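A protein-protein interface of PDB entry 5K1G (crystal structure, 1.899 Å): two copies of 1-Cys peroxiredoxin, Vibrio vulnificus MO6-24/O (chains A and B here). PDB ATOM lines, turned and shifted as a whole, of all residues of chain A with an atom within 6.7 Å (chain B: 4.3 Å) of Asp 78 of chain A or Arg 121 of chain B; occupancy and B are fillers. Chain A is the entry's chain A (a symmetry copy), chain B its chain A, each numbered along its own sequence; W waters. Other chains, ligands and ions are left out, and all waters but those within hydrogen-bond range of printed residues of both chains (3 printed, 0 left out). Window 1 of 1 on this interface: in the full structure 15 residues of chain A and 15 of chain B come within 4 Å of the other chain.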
ATOM      1  N   SER A  14       5.177 -24.875  24.865  1.00  0.00           N
ATOM      2  CA  SER A  14       6.453 -25.380  25.348  1.00  0.00           C
ATOM      3  C   SER A  14       7.494 -24.272  25.444  1.00  0.00           C
ATOM      4  O   SER A  14       7.449 -23.277  24.716  1.00  0.00           O
ATOM      5  CB  SER A  14       6.965 -26.500  24.439  1.00  0.00           C
ATOM      6  OG  SER A  14       5.989 -27.522  24.308  1.00  0.00           O
ATOM      7  N   SER A  75       4.690 -18.592  18.736  1.00  0.00           N
ATOM      8  CA  SER A  75       4.871 -18.805  17.310  1.00  0.00           C
ATOM      9  C   SER A  75       4.777 -20.293  17.028  1.00  0.00           C
ATOM     10  O   SER A  75       5.049 -21.126  17.896  1.00  0.00           O
ATOM     11  CB  SER A  75       6.213 -18.257  16.815  1.00  0.00           C
ATOM     12  OG  SER A  75       6.310 -18.382  15.405  1.00  0.00           O
ATOM     13  N   VAL A  76       4.374 -20.619  15.803  1.00  0.00           N
ATOM     14  CA  VAL A  76       4.434 -22.000  15.349  1.00  0.00           C
ATOM     15  C   VAL A  76       5.878 -22.268  14.953  1.00  0.00           C
ATOM     16  O   VAL A  76       6.229 -22.270  13.768  1.00  0.00           O
ATOM     17  CB  VAL A  76       3.447 -22.277  14.201  1.00  0.00           C
ATOM     18  CG1 VAL A  76       3.502 -23.744  13.786  1.00  0.00           C
ATOM     19  CG2 VAL A  76       2.037 -21.913  14.632  1.00  0.00           C
ATOM     20  N   ASN A  77       6.729 -22.422  15.963  1.00  0.00           N
ATOM     21  CA  ASN A  77       8.109 -22.851  15.823  1.00  0.00           C
ATOM     22  C   ASN A  77       8.398 -23.807  16.969  1.00  0.00           C
ATOM     23  O   ASN A  77       7.633 -23.887  17.933  1.00  0.00           O
ATOM     24  CB  ASN A  77       9.095 -21.671  15.867  1.00  0.00           C
ATOM     25  CG  ASN A  77       9.049 -20.813  14.617  1.00  0.00           C
ATOM     26  OD1 ASN A  77       8.385 -19.778  14.589  1.00  0.00           O
ATOM     27  ND2 ASN A  77       9.775 -21.227  13.586  1.00  0.00           N
ATOM     28  N   ASP A  78       9.511 -24.526  16.871  1.00  0.00           N
ATOM     29  CA  ASP A  78       9.895 -25.386  17.980  1.00  0.00           C
ATOM     30  C   ASP A  78      10.617 -24.571  19.054  1.00  0.00           C
ATOM     31  O   ASP A  78      11.019 -23.424  18.840  1.00  0.00           O
ATOM     32  CB  ASP A  78      10.770 -26.539  17.495  1.00  0.00           C
ATOM     33  CG  ASP A  78      12.064 -26.062  16.878  1.00  0.00           C
ATOM     34  OD1 ASP A  78      13.033 -25.836  17.633  1.00  0.00           O
ATOM     35  OD2 ASP A  78      12.109 -25.913  15.639  1.00  0.00           O
ATOM     36  N   ALA A  79      10.789 -25.187  20.227  1.00  0.00           N
ATOM     37  CA  ALA A  79      11.320 -24.460  21.375  1.00  0.00           C
ATOM     38  C   ALA A  79      12.792 -24.105  21.202  1.00  0.00           C
ATOM     39  O   ALA A  79      13.257 -23.116  21.781  1.00  0.00           O
ATOM     40  CB  ALA A  79      11.118 -25.274  22.653  1.00  0.00           C
ATOM     41  N   PHE A  80      13.539 -24.889  20.421  1.00  0.00           N
ATOM     42  CA  PHE A  80      14.944 -24.560  20.193  1.00  0.00           C
ATOM     43  C   PHE A  80      15.085 -23.321  19.319  1.00  0.00           C
ATOM     44  O   PHE A  80      15.947 -22.470  19.575  1.00  0.00           O
ATOM     45  CB  PHE A  80      15.672 -25.750  19.569  1.00  0.00           C
ATOM     46  CG  PHE A  80      15.901 -26.886  20.523  1.00  0.00           C
ATOM     47  CD1 PHE A  80      16.930 -26.831  21.449  1.00  0.00           C
ATOM     48  CD2 PHE A  80      15.089 -28.008  20.499  1.00  0.00           C
ATOM     49  CE1 PHE A  80      17.144 -27.871  22.336  1.00  0.00           C
ATOM     50  CE2 PHE A  80      15.300 -29.054  21.382  1.00  0.00           C
ATOM     51  CZ  PHE A  80      16.329 -28.983  22.303  1.00  0.00           C
ATOM     52  N   VAL A  81      14.250 -23.198  18.286  1.00  0.00           N
ATOM     53  CA  VAL A  81      14.268 -21.999  17.454  1.00  0.00           C
ATOM     54  C   VAL A  81      13.796 -20.791  18.254  1.00  0.00           C
ATOM     55  O   VAL A  81      14.369 -19.698  18.150  1.00  0.00           O
ATOM     56  CB  VAL A  81      13.420 -22.216  16.186  1.00  0.00           C
ATOM     57  CG1 VAL A  81      13.185 -20.897  15.458  1.00  0.00           C
ATOM     58  CG2 VAL A  81      14.099 -23.215  15.263  1.00  0.00           C
ATOM     59  N   MET A  82      12.756 -20.968  19.073  1.00  0.00           N
ATOM     60  CA  MET A  82      12.259 -19.858  19.880  1.00  0.00           C
ATOM     61  C   MET A  82      13.311 -19.383  20.875  1.00  0.00           C
ATOM     62  O   MET A  82      13.478 -18.176  21.080  1.00  0.00           O
ATOM     63  CB  MET A  82      10.976 -20.265  20.608  1.00  0.00           C
ATOM     64  CG  MET A  82       9.775 -20.495  19.691  1.00  0.00           C
ATOM     65  SD  MET A  82       9.314 -19.041  18.723  1.00  0.00           S
ATOM     66  CE  MET A  82       8.571 -17.999  19.979  1.00  0.00           C
ATOM     67  N   LYS A  83      14.036 -20.313  21.499  1.00  0.00           N
ATOM     68  CA  LYS A  83      15.075 -19.913  22.444  1.00  0.00           C
ATOM     69  C   LYS A  83      16.196 -19.163  21.736  1.00  0.00           C
ATOM     70  O   LYS A  83      16.656 -18.116  22.209  1.00  0.00           O
ATOM     71  CB  LYS A  83      15.632 -21.131  23.183  1.00  0.00           C
ATOM     72  CG  LYS A  83      16.549 -20.754  24.343  1.00  0.00           C
ATOM     73  CD  LYS A  83      17.324 -21.948  24.884  1.00  0.00           C
ATOM     74  CE  LYS A  83      18.710 -22.072  24.263  1.00  0.00           C
ATOM     75  NZ  LYS A  83      19.605 -20.953  24.673  1.00  0.00           N
ATOM     76  N   LEU A  97       7.043 -18.636  23.783  1.00  0.00           N
ATOM     77  CA  LEU A  97       6.340 -19.908  23.853  1.00  0.00           C
ATOM     78  C   LEU A  97       6.280 -20.539  22.468  1.00  0.00           C
ATOM     79  O   LEU A  97       6.106 -19.841  21.464  1.00  0.00           O
ATOM     80  CB  LEU A  97       4.927 -19.716  24.413  1.00  0.00           C
ATOM     81  CG  LEU A  97       4.889 -19.099  25.811  1.00  0.00           C
ATOM     82  CD1 LEU A  97       3.479 -18.654  26.177  1.00  0.00           C
ATOM     83  CD2 LEU A  97       5.438 -20.071  26.855  1.00  0.00           C
ATOM     84  N   ALA A  98       6.422 -21.859  22.420  1.00  0.00           N
ATOM     85  CA  ALA A  98       6.492 -22.594  21.165  1.00  0.00           C
ATOM     86  C   ALA A  98       5.224 -23.411  20.967  1.00  0.00           C
ATOM     87  O   ALA A  98       4.793 -24.135  21.871  1.00  0.00           O
ATOM     88  CB  ALA A  98       7.718 -23.507  21.135  1.00  0.00           C
ATOM     89  N   ASP A  99       4.633 -23.291  19.784  1.00  0.00           N
ATOM     90  CA  ASP A  99       3.473 -24.076  19.368  1.00  0.00           C
ATOM     91  C   ASP A  99       3.891 -24.925  18.168  1.00  0.00           C
ATOM     92  O   ASP A  99       3.408 -24.723  17.051  1.00  0.00           O
ATOM     93  CB  ASP A  99       2.290 -23.137  19.040  1.00  0.00           C
ATOM     94  CG  ASP A  99       1.000 -23.882  18.786  1.00  0.00           C
ATOM     95  OD1 ASP A  99       0.853 -25.013  19.296  1.00  0.00           O
ATOM     96  OD2 ASP A  99       0.123 -23.328  18.087  1.00  0.00           O
ATOM     97  N   GLY A 100       4.785 -25.890  18.417  1.00  0.00           N
ATOM     98  CA  GLY A 100       5.543 -26.503  17.332  1.00  0.00           C
ATOM     99  C   GLY A 100       4.680 -27.156  16.266  1.00  0.00           C
ATOM    100  O   GLY A 100       5.010 -27.113  15.078  1.00  0.00           O
ATOM    101  N   PRO B  41      16.354 -32.923  11.318  1.00  0.00           N
ATOM    102  CA  PRO B  41      14.969 -32.689  11.758  1.00  0.00           C
ATOM    103  C   PRO B  41      14.659 -31.228  12.034  1.00  0.00           C
ATOM    104  O   PRO B  41      13.494 -30.827  11.928  1.00  0.00           O
ATOM    105  CB  PRO B  41      14.856 -33.540  13.033  1.00  0.00           C
ATOM    106  CG  PRO B  41      15.951 -34.559  12.916  1.00  0.00           C
ATOM    107  CD  PRO B  41      17.068 -33.851  12.209  1.00  0.00           C
ATOM    108  N   GLY B  42      15.653 -30.417  12.382  1.00  0.00           N
ATOM    109  CA  GLY B  42      15.365 -29.027  12.666  1.00  0.00           C
ATOM    110  C   GLY B  42      16.574 -28.145  12.885  1.00  0.00           C
ATOM    111  O   GLY B  42      17.497 -28.505  13.622  1.00  0.00           O
ATOM    112  N   VAL B  76      13.056 -29.202   7.221  1.00  0.00           N
ATOM    113  CA  VAL B  76      11.701 -28.669   7.213  1.00  0.00           C
ATOM    114  C   VAL B  76      11.706 -27.452   8.125  1.00  0.00           C
ATOM    115  O   VAL B  76      11.263 -27.510   9.278  1.00  0.00           O
ATOM    116  CB  VAL B  76      10.662 -29.721   7.640  1.00  0.00           C
ATOM    117  CG1 VAL B  76       9.253 -29.143   7.575  1.00  0.00           C
ATOM    118  CG2 VAL B  76      10.763 -30.943   6.744  1.00  0.00           C
ATOM    119  N   ASN B  77      12.280 -26.363   7.622  1.00  0.00           N
ATOM    120  CA  ASN B  77      12.249 -25.050   8.243  1.00  0.00           C
ATOM    121  C   ASN B  77      12.049 -24.036   7.128  1.00  0.00           C
ATOM    122  O   ASN B  77      12.205 -24.355   5.948  1.00  0.00           O
ATOM    123  CB  ASN B  77      13.544 -24.734   9.009  1.00  0.00           C
ATOM    124  CG  ASN B  77      13.682 -25.531  10.292  1.00  0.00           C
ATOM    125  OD1 ASN B  77      14.352 -26.563  10.323  1.00  0.00           O
ATOM    126  ND2 ASN B  77      13.069 -25.044  11.364  1.00  0.00           N
ATOM    127  N   THR B 105      10.235 -33.306   1.364  1.00  0.00           N
ATOM    128  CA  THR B 105      10.429 -34.438   2.265  1.00  0.00           C
ATOM    129  C   THR B 105       9.327 -35.478   2.097  1.00  0.00           C
ATOM    130  O   THR B 105       9.598 -36.684   2.036  1.00  0.00           O
ATOM    131  CB  THR B 105      10.484 -33.939   3.710  1.00  0.00           C
ATOM    132  OG1 THR B 105      11.591 -33.043   3.864  1.00  0.00           O
ATOM    133  CG2 THR B 105      10.644 -35.098   4.677  1.00  0.00           C
ATOM    134  N   GLU B 111       9.404 -38.182   5.657  1.00  0.00           N
ATOM    135  CA  GLU B 111       8.914 -37.345   6.737  1.00  0.00           C
ATOM    136  C   GLU B 111       8.748 -38.165   8.013  1.00  0.00           C
ATOM    137  O   GLU B 111       8.743 -39.398   8.000  1.00  0.00           O
ATOM    138  CB  GLU B 111       7.582 -36.693   6.359  1.00  0.00           C
ATOM    139  CG  GLU B 111       6.386 -37.636   6.377  1.00  0.00           C
ATOM    140  CD  GLU B 111       6.197 -38.391   5.071  1.00  0.00           C
ATOM    141  OE1 GLU B 111       7.190 -38.610   4.343  1.00  0.00           O
ATOM    142  OE2 GLU B 111       5.042 -38.760   4.770  1.00  0.00           O
ATOM    143  N   MET B 112       8.624 -37.454   9.130  1.00  0.00           N
ATOM    144  CA  MET B 112       8.297 -38.077  10.403  1.00  0.00           C
ATOM    145  C   MET B 112       7.528 -37.075  11.247  1.00  0.00           C
ATOM    146  O   MET B 112       7.830 -35.878  11.234  1.00  0.00           O
ATOM    147  CB  MET B 112       9.550 -38.557  11.150  1.00  0.00           C
ATOM    148  CG  MET B 112      10.539 -37.463  11.501  1.00  0.00           C
ATOM    149  SD  MET B 112      11.802 -38.027  12.655  1.00  0.00           S
ATOM    150  CE  MET B 112      12.641 -36.484  13.005  1.00  0.00           C
ATOM    151  N   THR B 114       6.882 -35.386  14.465  1.00  0.00           N
ATOM    152  CA  THR B 114       7.417 -35.081  15.783  1.00  0.00           C
ATOM    153  C   THR B 114       6.341 -34.584  16.739  1.00  0.00           C
ATOM    154  O   THR B 114       6.670 -34.122  17.836  1.00  0.00           O
ATOM    155  CB  THR B 114       8.545 -34.050  15.679  1.00  0.00           C
ATOM    156  OG1 THR B 114       7.992 -32.758  15.403  1.00  0.00           O
ATOM    157  CG2 THR B 114       9.521 -34.436  14.569  1.00  0.00           C
ATOM    158  N   PHE B 117       6.386 -31.444  19.244  1.00  0.00           N
ATOM    159  CA  PHE B 117       7.686 -30.783  19.178  1.00  0.00           C
ATOM    160  C   PHE B 117       7.739 -29.777  18.035  1.00  0.00           C
ATOM    161  O   PHE B 117       8.041 -28.597  18.248  1.00  0.00           O
ATOM    162  CB  PHE B 117       8.817 -31.799  19.027  1.00  0.00           C
ATOM    163  CG  PHE B 117      10.125 -31.167  18.638  1.00  0.00           C
ATOM    164  CD1 PHE B 117      10.888 -30.490  19.579  1.00  0.00           C
ATOM    165  CD2 PHE B 117      10.574 -31.210  17.327  1.00  0.00           C
ATOM    166  CE1 PHE B 117      12.081 -29.889  19.224  1.00  0.00           C
ATOM    167  CE2 PHE B 117      11.764 -30.607  16.966  1.00  0.00           C
ATOM    168  CZ  PHE B 117      12.519 -29.947  17.916  1.00  0.00           C
ATOM    169  N   GLY B 118       7.477 -30.230  16.812  1.00  0.00           N
ATOM    170  CA  GLY B 118       7.572 -29.361  15.656  1.00  0.00           C
ATOM    171  C   GLY B 118       6.789 -29.862  14.462  1.00  0.00           C
ATOM    172  O   GLY B 118       7.120 -29.546  13.316  1.00  0.00           O
ATOM    173  N   GLY B 119       5.744 -30.640  14.723  1.00  0.00           N
ATOM    174  CA  GLY B 119       4.928 -31.175  13.654  1.00  0.00           C
ATOM    175  C   GLY B 119       5.733 -32.077  12.737  1.00  0.00           C
ATOM    176  O   GLY B 119       6.672 -32.767  13.155  1.00  0.00           O
ATOM    177  N   LEU B 120       5.362 -32.062  11.459  1.00  0.00           N
ATOM    178  CA  LEU B 120       6.070 -32.852  10.459  1.00  0.00           C
ATOM    179  C   LEU B 120       7.466 -32.290  10.225  1.00  0.00           C
ATOM    180  O   LEU B 120       7.626 -31.110   9.892  1.00  0.00           O
ATOM    181  CB  LEU B 120       5.291 -32.869   9.146  1.00  0.00           C
ATOM    182  CG  LEU B 120       4.132 -33.849   8.960  1.00  0.00           C
ATOM    183  CD1 LEU B 120       3.684 -33.844   7.504  1.00  0.00           C
ATOM    184  CD2 LEU B 120       4.513 -35.257   9.403  1.00  0.00           C
ATOM    185  N   ARG B 121       8.476 -33.138  10.390  1.00  0.00           N
ATOM    186  CA  ARG B 121       9.856 -32.792  10.094  1.00  0.00           C
ATOM    187  C   ARG B 121      10.439 -33.869   9.188  1.00  0.00           C
ATOM    188  O   ARG B 121       9.775 -34.851   8.844  1.00  0.00           O
ATOM    189  CB  ARG B 121      10.684 -32.642  11.377  1.00  0.00           C
ATOM    190  CG  ARG B 121      10.183 -31.551  12.309  1.00  0.00           C
ATOM    191  CD  ARG B 121      10.278 -30.180  11.658  1.00  0.00           C
ATOM    192  NE  ARG B 121       9.861 -29.112  12.561  1.00  0.00           N
ATOM    193  CZ  ARG B 121      10.702 -28.332  13.232  1.00  0.00           C
ATOM    194  NH1 ARG B 121      12.011 -28.503  13.106  1.00  0.00           N
ATOM    195  NH2 ARG B 121      10.236 -27.383  14.032  1.00  0.00           N
ATOM    196  N   SER B 122      11.689 -33.681   8.787  1.00  0.00           N
ATOM    197  CA  SER B 122      12.381 -34.689   8.003  1.00  0.00           C
ATOM    198  C   SER B 122      13.047 -35.700   8.924  1.00  0.00           C
ATOM    199  O   SER B 122      13.553 -35.346   9.994  1.00  0.00           O
ATOM    200  CB  SER B 122      13.431 -34.047   7.096  1.00  0.00           C
ATOM    201  OG  SER B 122      14.102 -35.037   6.338  1.00  0.00           O
ATOM    202  N   GLN B 123      13.031 -36.964   8.513  1.00  0.00           N
ATOM    203  CA  GLN B 123      13.951 -37.914   9.115  1.00  0.00           C
ATOM    204  C   GLN B 123      15.382 -37.488   8.812  1.00  0.00           C
ATOM    205  O   GLN B 123      15.655 -36.775   7.839  1.00  0.00           O
ATOM    206  CB  GLN B 123      13.713 -39.328   8.590  1.00  0.00           C
ATOM    207  CG  GLN B 123      12.329 -39.884   8.844  1.00  0.00           C
ATOM    208  CD  GLN B 123      12.155 -41.256   8.230  1.00  0.00           C
ATOM    209  OE1 GLN B 123      13.046 -42.102   8.317  1.00  0.00           O
ATOM    210  NE2 GLN B 123      11.013 -41.480   7.595  1.00  0.00           N
HETATM  211  O   HOH W   1       8.905 -27.325  20.674  1.00  0.00           O
HETATM  212  O   HOH W   2       7.473 -26.243  14.050  1.00  0.00           O
HETATM  213  O   HOH W   3      13.798 -26.403  13.833  1.00  0.00           O
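The side-chain carboxylate of Asp 78 of chain A lies within salt-bridge range of the guanidinium group of Arg 121 of chain B (2.9 Å).
The backbone NH of Met 112 of chain B sits at hydrogen-bond distance from the backbone carbonyl oxygen of Arg 121 of chain B (2.9 Å). The backbone carbonyl oxygen of Gly 119 of chain B sits at hydrogen-bond distance from the side-chain hydroxyl of Thr 114 of chain B, at 2.6 Å. The side-chain carboxylate (OD1) of Asp 78 of chain A sits at hydrogen-bond distance from the backbone NH (N) of Val 81 of chain A. OD1 of Asp 78 of chain A is in hydrogen-bond range of N of Phe 80 of chain A, at 3.0 Å. NE of Arg 121 of chain B sits at hydrogen-bond distance from O of Gly 118 of chain B, at 2.9 Å. N of Gly 118 of chain B sits at hydrogen-bond distance from OG1 of Thr 114 of chain B.
Among the printed residues, merely in contact across the chains: Gly 100 of chain A with Gly 118 of chain B (3.3 Å), Gly 100 of chain A with Phe 117 of chain B (3.4 Å), Asp 78 of chain A with Phe 117 of chain B (3.5 Å), Gly 100 of chain A with Gly 119 of chain B (3.6 Å) and Phe 80 of chain A with Phe 117 of chain B (3.8 Å).
Asp 78 of chain A touches just these residues of chain B: Phe 117 and Arg 121. Arg 121 of chain B touches just one residue of chain A: Asp 78. Printed residues of chain A within 4 Å of Gly 118 of chain B: Gly 100 (3.3 Å). Of the printed residues of chain A, Gly 119 of chain B touches Gly 100. Printed residues of chain A within 4 Å of Phe 117 of chain B: Asp 78 (3.5 Å), Phe 80 (3.8 Å) and Gly 100 (3.4 Å). Of the printed residues of chain B, Gly 100 of chain A touches Phe 117, Gly 118 and Gly 119. The nearest printed residue of chain B that does not touch Asp 78 of chain A is Asn 77 of chain B (4.5 Å).
Of the 14 printed residues of chain A, 3 touch a printed residue of chain B. Printed residues of chain A that touch a printed residue of chain B: Asp 78, Phe 80 and Gly 100. Hydrophobic or aromatic side chains of chain A that line the printed part of chain B: Phe 80. Hydrophobic or aromatic side chains of chain B within 4 Å of the printed part of chain A: Phe 117. Along chain B the printed residues that touch a printed residue of chain A span positions 117 to 121. Among the printed residues, 6 pairs touch across the chains.
2 positions are printed for both chains. Of the 6 pairs that touch across the chains among the printed residues, none has its exchanged pair printed and touching as well.
Water W3 lies within hydrogen-bond range of OD2 of Asp 78 of chain A, NH1 of Arg 121 of chain B and ND2 of Asn 77 of chain B. Water W2 lies within hydrogen-bond range of O of Gly 100 of chain A (2.8 Å), NH2 of Arg 121 of chain B (3.0 Å) and O of Gly 118 of chain B (3.4 Å). Water W1 bridges the backbone carbonyl oxygen (O) of Phe 117 of chain B (2.9 Å) and the backbone NH (N) of Ala 79 of chain A (2.9 Å).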
